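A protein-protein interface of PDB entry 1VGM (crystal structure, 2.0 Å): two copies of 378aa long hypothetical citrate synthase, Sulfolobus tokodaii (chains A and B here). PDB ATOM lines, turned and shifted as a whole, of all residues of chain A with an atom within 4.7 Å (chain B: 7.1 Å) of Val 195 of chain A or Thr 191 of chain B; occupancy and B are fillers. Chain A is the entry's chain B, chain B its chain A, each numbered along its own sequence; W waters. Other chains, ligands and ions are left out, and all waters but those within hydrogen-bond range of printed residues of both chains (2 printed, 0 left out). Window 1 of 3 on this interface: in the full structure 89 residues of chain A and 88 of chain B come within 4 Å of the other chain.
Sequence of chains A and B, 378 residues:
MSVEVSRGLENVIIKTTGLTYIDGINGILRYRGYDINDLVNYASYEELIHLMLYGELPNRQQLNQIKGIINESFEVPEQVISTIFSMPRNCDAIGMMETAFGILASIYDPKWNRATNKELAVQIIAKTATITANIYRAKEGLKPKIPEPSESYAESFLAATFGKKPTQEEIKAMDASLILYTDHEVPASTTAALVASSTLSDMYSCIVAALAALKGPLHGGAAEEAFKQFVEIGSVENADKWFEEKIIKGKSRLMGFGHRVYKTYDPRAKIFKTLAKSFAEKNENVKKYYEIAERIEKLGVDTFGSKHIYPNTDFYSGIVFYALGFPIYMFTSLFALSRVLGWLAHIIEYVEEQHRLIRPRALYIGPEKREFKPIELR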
ATOM      1  N   THR A 191      16.929  20.869   9.567  1.00  0.00           N
ATOM      2  CA  THR A 191      17.900  20.893  10.649  1.00  0.00           C
ATOM      3  C   THR A 191      19.118  21.734  10.270  1.00  0.00           C
ATOM      4  O   THR A 191      19.534  22.607  11.027  1.00  0.00           O
ATOM      5  CB  THR A 191      18.331  19.464  11.007  1.00  0.00           C
ATOM      6  OG1 THR A 191      17.182  18.739  11.476  1.00  0.00           O
ATOM      7  CG2 THR A 191      19.403  19.478  12.093  1.00  0.00           C
ATOM      8  N   ALA A 192      19.671  21.478   9.090  1.00  0.00           N
ATOM      9  CA  ALA A 192      20.829  22.229   8.622  1.00  0.00           C
ATOM     10  C   ALA A 192      20.507  23.726   8.580  1.00  0.00           C
ATOM     11  O   ALA A 192      21.299  24.547   9.037  1.00  0.00           O
ATOM     12  CB  ALA A 192      21.260  21.734   7.229  1.00  0.00           C
ATOM     13  N   ALA A 193      19.343  24.076   8.042  1.00  0.00           N
ATOM     14  CA  ALA A 193      18.912  25.471   8.002  1.00  0.00           C
ATOM     15  C   ALA A 193      18.865  26.102   9.399  1.00  0.00           C
ATOM     16  O   ALA A 193      19.334  27.226   9.599  1.00  0.00           O
ATOM     17  CB  ALA A 193      17.539  25.577   7.333  1.00  0.00           C
ATOM     18  N   LEU A 194      18.301  25.380  10.363  1.00  0.00           N
ATOM     19  CA  LEU A 194      18.260  25.863  11.740  1.00  0.00           C
ATOM     20  C   LEU A 194      19.653  26.045  12.342  1.00  0.00           C
ATOM     21  O   LEU A 194      19.905  27.035  13.045  1.00  0.00           O
ATOM     22  CB  LEU A 194      17.440  24.906  12.616  1.00  0.00           C
ATOM     23  CG  LEU A 194      15.929  24.964  12.387  1.00  0.00           C
ATOM     24  CD1 LEU A 194      15.269  23.745  13.007  1.00  0.00           C
ATOM     25  CD2 LEU A 194      15.373  26.249  12.980  1.00  0.00           C
ATOM     26  N   VAL A 195      20.558  25.103  12.075  1.00  0.00           N
ATOM     27  CA  VAL A 195      21.920  25.231  12.573  1.00  0.00           C
ATOM     28  C   VAL A 195      22.563  26.506  12.019  1.00  0.00           C
ATOM     29  O   VAL A 195      23.213  27.250  12.756  1.00  0.00           O
ATOM     30  CB  VAL A 195      22.778  23.990  12.200  1.00  0.00           C
ATOM     31  CG1 VAL A 195      24.256  24.264  12.478  1.00  0.00           C
ATOM     32  CG2 VAL A 195      22.328  22.785  13.025  1.00  0.00           C
ATOM     33  N   ALA A 196      22.360  26.769  10.732  1.00  0.00           N
ATOM     34  CA  ALA A 196      22.892  27.982  10.108  1.00  0.00           C
ATOM     35  C   ALA A 196      22.248  29.243  10.692  1.00  0.00           C
ATOM     36  O   ALA A 196      22.926  30.236  10.954  1.00  0.00           O
ATOM     37  CB  ALA A 196      22.673  27.933   8.595  1.00  0.00           C
ATOM     38  N   SER A 197      20.937  29.198  10.902  1.00  0.00           N
ATOM     39  CA  SER A 197      20.241  30.337  11.481  1.00  0.00           C
ATOM     40  C   SER A 197      20.672  30.589  12.926  1.00  0.00           C
ATOM     41  O   SER A 197      20.581  31.714  13.407  1.00  0.00           O
ATOM     42  CB  SER A 197      18.728  30.126  11.428  1.00  0.00           C
ATOM     43  OG  SER A 197      18.304  29.297  12.495  1.00  0.00           O
ATOM     44  N   SER A 198      21.148  29.561  13.621  1.00  0.00           N
ATOM     45  CA  SER A 198      21.525  29.752  15.019  1.00  0.00           C
ATOM     46  C   SER A 198      22.761  30.637  15.158  1.00  0.00           C
ATOM     47  O   SER A 198      23.017  31.190  16.233  1.00  0.00           O
ATOM     48  CB  SER A 198      21.765  28.408  15.715  1.00  0.00           C
ATOM     49  OG  SER A 198      23.057  27.906  15.442  1.00  0.00           O
ATOM     50  N   THR A 199      23.517  30.785  14.072  1.00  0.00           N
ATOM     51  CA  THR A 199      24.670  31.688  14.073  1.00  0.00           C
ATOM     52  C   THR A 199      24.308  33.029  13.449  1.00  0.00           C
ATOM     53  O   THR A 199      25.156  33.902  13.311  1.00  0.00           O
ATOM     54  CB  THR A 199      25.861  31.087  13.295  1.00  0.00           C
ATOM     55  OG1 THR A 199      25.589  31.113  11.886  1.00  0.00           O
ATOM     56  CG2 THR A 199      26.107  29.656  13.739  1.00  0.00           C
ATOM     57  N   ILE A 358      23.702  26.935  18.247  1.00  0.00           N
ATOM     58  CA  ILE A 358      23.775  25.485  18.318  1.00  0.00           C
ATOM     59  C   ILE A 358      25.232  25.014  18.349  1.00  0.00           C
ATOM     60  O   ILE A 358      26.031  25.366  17.475  1.00  0.00           O
ATOM     61  CB  ILE A 358      23.028  24.839  17.127  1.00  0.00           C
ATOM     62  CG1 ILE A 358      21.516  25.091  17.274  1.00  0.00           C
ATOM     63  CG2 ILE A 358      23.323  23.351  17.065  1.00  0.00           C
ATOM     64  CD1 ILE A 358      20.665  24.594  16.106  1.00  0.00           C
ATOM     65  N   PRO A 360      26.732  21.261  19.807  1.00  0.00           N
ATOM     66  CA  PRO A 360      26.687  19.982  20.529  1.00  0.00           C
ATOM     67  C   PRO A 360      28.074  19.508  20.957  1.00  0.00           C
ATOM     68  O   PRO A 360      29.079  20.173  20.694  1.00  0.00           O
ATOM     69  CB  PRO A 360      26.037  19.031  19.524  1.00  0.00           C
ATOM     70  CG  PRO A 360      26.475  19.591  18.179  1.00  0.00           C
ATOM     71  CD  PRO A 360      26.486  21.092  18.360  1.00  0.00           C
ATOM     72  N   LEU B   9      21.441  22.432  21.749  1.00  0.00           N
ATOM     73  CA  LEU B   9      21.976  21.066  21.765  1.00  0.00           C
ATOM     74  C   LEU B   9      23.231  20.919  22.638  1.00  0.00           C
ATOM     75  O   LEU B   9      24.013  19.992  22.465  1.00  0.00           O
ATOM     76  CB  LEU B   9      22.284  20.608  20.338  1.00  0.00           C
ATOM     77  CG  LEU B   9      21.159  20.640  19.304  1.00  0.00           C
ATOM     78  CD1 LEU B   9      21.696  20.234  17.940  1.00  0.00           C
ATOM     79  CD2 LEU B   9      20.074  19.699  19.722  1.00  0.00           C
ATOM     80  N   ILE B  14      26.680  14.468  19.842  1.00  0.00           N
ATOM     81  CA  ILE B  14      26.255  14.191  18.476  1.00  0.00           C
ATOM     82  C   ILE B  14      27.115  13.105  17.833  1.00  0.00           C
ATOM     83  O   ILE B  14      26.697  12.459  16.877  1.00  0.00           O
ATOM     84  CB  ILE B  14      26.295  15.471  17.588  1.00  0.00           C
ATOM     85  CG1 ILE B  14      25.616  15.179  16.243  1.00  0.00           C
ATOM     86  CG2 ILE B  14      27.735  15.948  17.386  1.00  0.00           C
ATOM     87  CD1 ILE B  14      25.471  16.391  15.349  1.00  0.00           C
ATOM     88  N   VAL B 186      32.684  21.138  18.688  1.00  0.00           N
ATOM     89  CA  VAL B 186      31.783  20.915  17.565  1.00  0.00           C
ATOM     90  C   VAL B 186      30.890  22.132  17.400  1.00  0.00           C
ATOM     91  O   VAL B 186      29.715  22.113  17.771  1.00  0.00           O
ATOM     92  CB  VAL B 186      30.897  19.671  17.785  1.00  0.00           C
ATOM     93  CG1 VAL B 186      30.297  19.233  16.468  1.00  0.00           C
ATOM     94  CG2 VAL B 186      31.715  18.543  18.388  1.00  0.00           C
ATOM     95  N   PRO B 187      31.450  23.220  16.855  1.00  0.00           N
ATOM     96  CA  PRO B 187      30.670  24.435  16.612  1.00  0.00           C
ATOM     97  C   PRO B 187      29.645  24.219  15.508  1.00  0.00           C
ATOM     98  O   PRO B 187      29.498  23.111  14.990  1.00  0.00           O
ATOM     99  CB  PRO B 187      31.735  25.466  16.226  1.00  0.00           C
ATOM    100  CG  PRO B 187      32.809  24.639  15.590  1.00  0.00           C
ATOM    101  CD  PRO B 187      32.848  23.372  16.409  1.00  0.00           C
ATOM    102  N   ALA B 188      28.947  25.287  15.140  1.00  0.00           N
ATOM    103  CA  ALA B 188      27.808  25.174  14.236  1.00  0.00           C
ATOM    104  C   ALA B 188      28.240  24.725  12.840  1.00  0.00           C
ATOM    105  O   ALA B 188      27.523  23.967  12.173  1.00  0.00           O
ATOM    106  CB  ALA B 188      27.079  26.503  14.161  1.00  0.00           C
ATOM    107  N   SER B 189      29.413  25.172  12.397  1.00  0.00           N
ATOM    108  CA  SER B 189      29.914  24.735  11.095  1.00  0.00           C
ATOM    109  C   SER B 189      30.134  23.233  11.057  1.00  0.00           C
ATOM    110  O   SER B 189      29.604  22.550  10.183  1.00  0.00           O
ATOM    111  CB  SER B 189      31.214  25.461  10.727  1.00  0.00           C
ATOM    112  OG  SER B 189      32.186  25.352  11.750  1.00  0.00           O
ATOM    113  N   THR B 190      30.908  22.709  11.999  1.00  0.00           N
ATOM    114  CA  THR B 190      31.102  21.265  12.077  1.00  0.00           C
ATOM    115  C   THR B 190      29.753  20.535  12.192  1.00  0.00           C
ATOM    116  O   THR B 190      29.561  19.467  11.615  1.00  0.00           O
ATOM    117  CB  THR B 190      31.992  20.903  13.281  1.00  0.00           C
ATOM    118  OG1 THR B 190      33.203  21.665  13.217  1.00  0.00           O
ATOM    119  CG2 THR B 190      32.340  19.416  13.271  1.00  0.00           C
ATOM    120  N   THR B 191      28.814  21.120  12.931  1.00  0.00           N
ATOM    121  CA  THR B 191      27.505  20.491  13.120  1.00  0.00           C
ATOM    122  C   THR B 191      26.761  20.414  11.788  1.00  0.00           C
ATOM    123  O   THR B 191      26.189  19.381  11.441  1.00  0.00           O
ATOM    124  CB  THR B 191      26.646  21.283  14.143  1.00  0.00           C
ATOM    125  OG1 THR B 191      27.366  21.399  15.377  1.00  0.00           O
ATOM    126  CG2 THR B 191      25.302  20.583  14.398  1.00  0.00           C
ATOM    127  N   ALA B 192      26.780  21.508  11.037  1.00  0.00           N
ATOM    128  CA  ALA B 192      26.074  21.559   9.764  1.00  0.00           C
ATOM    129  C   ALA B 192      26.678  20.562   8.765  1.00  0.00           C
ATOM    130  O   ALA B 192      25.955  19.928   8.000  1.00  0.00           O
ATOM    131  CB  ALA B 192      26.121  22.986   9.197  1.00  0.00           C
ATOM    132  N   ALA B 193      27.999  20.414   8.772  1.00  0.00           N
ATOM    133  CA  ALA B 193      28.634  19.425   7.895  1.00  0.00           C
ATOM    134  C   ALA B 193      28.219  17.997   8.270  1.00  0.00           C
ATOM    135  O   ALA B 193      27.939  17.167   7.408  1.00  0.00           O
ATOM    136  CB  ALA B 193      30.153  19.558   7.962  1.00  0.00           C
ATOM    137  N   LEU B 194      28.192  17.711   9.562  1.00  0.00           N
ATOM    138  CA  LEU B 194      27.748  16.407  10.021  1.00  0.00           C
ATOM    139  C   LEU B 194      26.306  16.137   9.594  1.00  0.00           C
ATOM    140  O   LEU B 194      25.975  15.038   9.134  1.00  0.00           O
ATOM    141  CB  LEU B 194      27.870  16.318  11.541  1.00  0.00           C
ATOM    142  CG  LEU B 194      29.317  16.199  12.014  1.00  0.00           C
ATOM    143  CD1 LEU B 194      29.401  16.427  13.527  1.00  0.00           C
ATOM    144  CD2 LEU B 194      29.859  14.835  11.621  1.00  0.00           C
ATOM    145  N   VAL B 195      25.451  17.145   9.741  1.00  0.00           N
ATOM    146  CA  VAL B 195      24.053  16.985   9.387  1.00  0.00           C
ATOM    147  C   VAL B 195      23.909  16.640   7.904  1.00  0.00           C
ATOM    148  O   VAL B 195      23.107  15.784   7.538  1.00  0.00           O
ATOM    149  CB  VAL B 195      23.246  18.266   9.705  1.00  0.00           C
ATOM    150  CG1 VAL B 195      21.842  18.163   9.119  1.00  0.00           C
ATOM    151  CG2 VAL B 195      23.172  18.470  11.208  1.00  0.00           C
ATOM    152  N   ALA B 196      24.695  17.296   7.055  1.00  0.00           N
ATOM    153  CA  ALA B 196      24.703  16.975   5.626  1.00  0.00           C
ATOM    154  C   ALA B 196      25.299  15.591   5.354  1.00  0.00           C
ATOM    155  O   ALA B 196      24.816  14.857   4.491  1.00  0.00           O
ATOM    156  CB  ALA B 196      25.481  18.037   4.854  1.00  0.00           C
ATOM    157  N   SER B 197      26.358  15.230   6.072  1.00  0.00           N
ATOM    158  CA  SER B 197      26.995  13.942   5.816  1.00  0.00           C
ATOM    159  C   SER B 197      26.046  12.820   6.228  1.00  0.00           C
ATOM    160  O   SER B 197      26.093  11.723   5.675  1.00  0.00           O
ATOM    161  CB  SER B 197      28.307  13.813   6.589  1.00  0.00           C
ATOM    162  OG  SER B 197      28.055  13.565   7.959  1.00  0.00           O
ATOM    163  N   ALA B 209      27.748  23.229   3.601  1.00  0.00           N
ATOM    164  CA  ALA B 209      26.897  23.391   4.776  1.00  0.00           C
ATOM    165  C   ALA B 209      27.664  24.052   5.922  1.00  0.00           C
ATOM    166  O   ALA B 209      27.189  25.023   6.518  1.00  0.00           O
ATOM    167  CB  ALA B 209      26.361  22.028   5.214  1.00  0.00           C
ATOM    168  N   ALA B 210      28.855  23.529   6.220  1.00  0.00           N
ATOM    169  CA  ALA B 210      29.716  24.100   7.256  1.00  0.00           C
ATOM    170  C   ALA B 210      29.920  25.594   7.027  1.00  0.00           C
ATOM    171  O   ALA B 210      29.861  26.399   7.957  1.00  0.00           O
ATOM    172  CB  ALA B 210      31.081  23.384   7.268  1.00  0.00           C
ATOM    173  N   ALA B 212      28.124  27.754   5.339  1.00  0.00           N
ATOM    174  CA  ALA B 212      26.906  28.535   5.530  1.00  0.00           C
ATOM    175  C   ALA B 212      26.679  28.875   7.015  1.00  0.00           C
ATOM    176  O   ALA B 212      26.319  29.999   7.366  1.00  0.00           O
ATOM    177  CB  ALA B 212      25.712  27.770   4.967  1.00  0.00           C
ATOM    178  N   ALA B 213      26.909  27.898   7.883  1.00  0.00           N
ATOM    179  CA  ALA B 213      26.889  28.132   9.323  1.00  0.00           C
ATOM    180  C   ALA B 213      27.993  29.087   9.776  1.00  0.00           C
ATOM    181  O   ALA B 213      27.765  29.954  10.620  1.00  0.00           O
ATOM    182  CB  ALA B 213      27.014  26.804  10.059  1.00  0.00           C
ATOM    183  N   TRP B 343      36.700  19.609   9.648  1.00  0.00           N
ATOM    184  CA  TRP B 343      35.403  19.269   9.068  1.00  0.00           C
ATOM    185  C   TRP B 343      35.459  17.930   8.326  1.00  0.00           C
ATOM    186  O   TRP B 343      34.604  17.064   8.530  1.00  0.00           O
ATOM    187  CB  TRP B 343      34.912  20.363   8.109  1.00  0.00           C
ATOM    188  CG  TRP B 343      34.547  21.669   8.783  1.00  0.00           C
ATOM    189  CD1 TRP B 343      34.111  21.846  10.075  1.00  0.00           C
ATOM    190  CD2 TRP B 343      34.596  22.979   8.196  1.00  0.00           C
ATOM    191  NE1 TRP B 343      33.891  23.183  10.323  1.00  0.00           N
ATOM    192  CE2 TRP B 343      34.181  23.901   9.188  1.00  0.00           C
ATOM    193  CE3 TRP B 343      34.975  23.465   6.939  1.00  0.00           C
ATOM    194  CZ2 TRP B 343      34.136  25.286   8.956  1.00  0.00           C
ATOM    195  CZ3 TRP B 343      34.930  24.840   6.707  1.00  0.00           C
ATOM    196  CH2 TRP B 343      34.514  25.735   7.712  1.00  0.00           C
ATOM    197  N   ILE B 358      20.197  11.995  10.339  1.00  0.00           N
ATOM    198  CA  ILE B 358      19.805  12.883  11.422  1.00  0.00           C
ATOM    199  C   ILE B 358      18.413  13.478  11.201  1.00  0.00           C
ATOM    200  O   ILE B 358      18.108  13.998  10.126  1.00  0.00           O
ATOM    201  CB  ILE B 358      20.846  14.003  11.608  1.00  0.00           C
ATOM    202  CG1 ILE B 358      22.158  13.384  12.117  1.00  0.00           C
ATOM    203  CG2 ILE B 358      20.333  15.057  12.602  1.00  0.00           C
ATOM    204  CD1 ILE B 358      23.304  14.370  12.283  1.00  0.00           C
HETATM  205  O   HOH W   1      28.570  26.976  17.403  1.00  0.00           O
HETATM  206  O   HOH W   2      31.169  22.047  20.664  1.00  0.00           O
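The backbone carbonyl oxygen (O) of Ala 213 of chain B is in hydrogen-bond range of the side-chain hydroxyl (OG1) of Thr 199 of chain A, at 2.8 Å.
The side-chain hydroxyl (OG1) of Thr 191 of chain B sits at hydrogen-bond distance from the backbone carbonyl oxygen (O) of Val 186 of chain B (3.4 Å).
O of Pro 187 of chain B sits at hydrogen-bond distance from OG1 of Thr 191 of chain B.
The side-chain hydroxyl (OG) of Ser 198 of chain A lies within hydrogen-bond range of the backbone carbonyl oxygen (O) of Val 195 of chain A, 2.8 Å away.
O of Ala 196 of chain A lies within hydrogen-bond range of OG1 of Thr 199 of chain A, 3.0 Å away.
OG of Ser 198 of chain A sits at hydrogen-bond distance from N of Ile 358 of chain A.
Ala 192 of chain A touches Val 195 of chain B.
Val 195 of chain A touches Ala 188 of chain B.
Thr 191 of chain B touches Val 195 of chain A.
Ala 188 of chain B touches Thr 199 of chain A (CB to CG2, 3.3 Å).
Ile 358 of chain A touches Leu 9 of chain B (CG2 to CD1, 3.6 Å).
CB of Ala 188 of chain B touches O of Ile 358 of chain A (3.7 Å).
Pro 360 of chain A touches Leu 9 of chain B (CA to O, 3.3 Å).
CG of Pro 360 of chain A touches CG2 of Ile 14 of chain B, at 3.9 Å.
Pro 360 of chain A touches Val 186 of chain B (CD to O, 3.4 Å).
Thr 191 of chain B touches Pro 360 of chain A (OG1 to CD, 3.1 Å).
Of the printed residues of chain B, Val 195 of chain A touches Ala 188 (3.3 Å), Thr 191 (3.9 Å) and Ala 192 (3.98 Å).
Ala 196 of chain A touches none of the printed residues of chain B.
Printed residues of chain B within 4 Å of Ile 358 of chain A: Leu 9 (3.6 Å) and Ala 188 (3.7 Å).
Of the printed residues of chain A, Leu 9 of chain B touches Ile 358 and Pro 360.
Printed residues of chain A within 4 Å of Ile 14 of chain B: Pro 360.
Printed residues of chain A within 4 Å of Val 186 of chain B: Pro 360 (3.4 Å).
Thr 191 of chain B touches just these residues of chain A: Val 195 (3.9 Å) and Pro 360 (3.1 Å).
The nearest residue of chain A that does not touch Thr 191 of chain B is Ile 358 of chain A (4.3 Å).
The nearest printed residue of chain B that does not touch Thr 199 of chain A is Ala 212 of chain B (4.7 Å).
Printed residues of chain A that touch a printed residue of chain B: Ala 192, Val 195, Thr 199, Ile 358 and Pro 360.
Printed residues of chain B that touch a printed residue of chain A: Leu 9, Ile 14, Val 186, Ala 188, Thr 191, Ala 192, Val 195 and Ala 213.
Hydrophobic or aromatic side chains of chain B that line the printed part of chain A: Leu 9, Ile 14, Val 186, Ala 188, Ala 192 and Val 195.
Among the printed residues, no Asp or Glu carboxylate lies within 4 Å of a Lys or Arg side-chain nitrogen of the other chain.
Ala 192 of chain A touches Val 195 of chain B, and with the chains exchanged Val 195 of chain A touches Ala 192 of chain B.
Val 195 of chain A touches Thr 191 of chain B, but with the chains exchanged Thr 191 of chain A does not touch Val 195 of chain B (4.001 Å).
Of the 12 pairs that touch across the chains among the printed residues, 2 have their exchanged pair printed and touching as well.
Water W2 bridges the backbone NH of Val 186 of chain B (2.7 Å) and the backbone carbonyl oxygen of Pro 360 of chain A (2.8 Å).
Water W1 bridges the backbone NH of Ala 188 of chain B (2.8 Å) and the backbone carbonyl oxygen of Ile 358 of chain A (3.0 Å).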
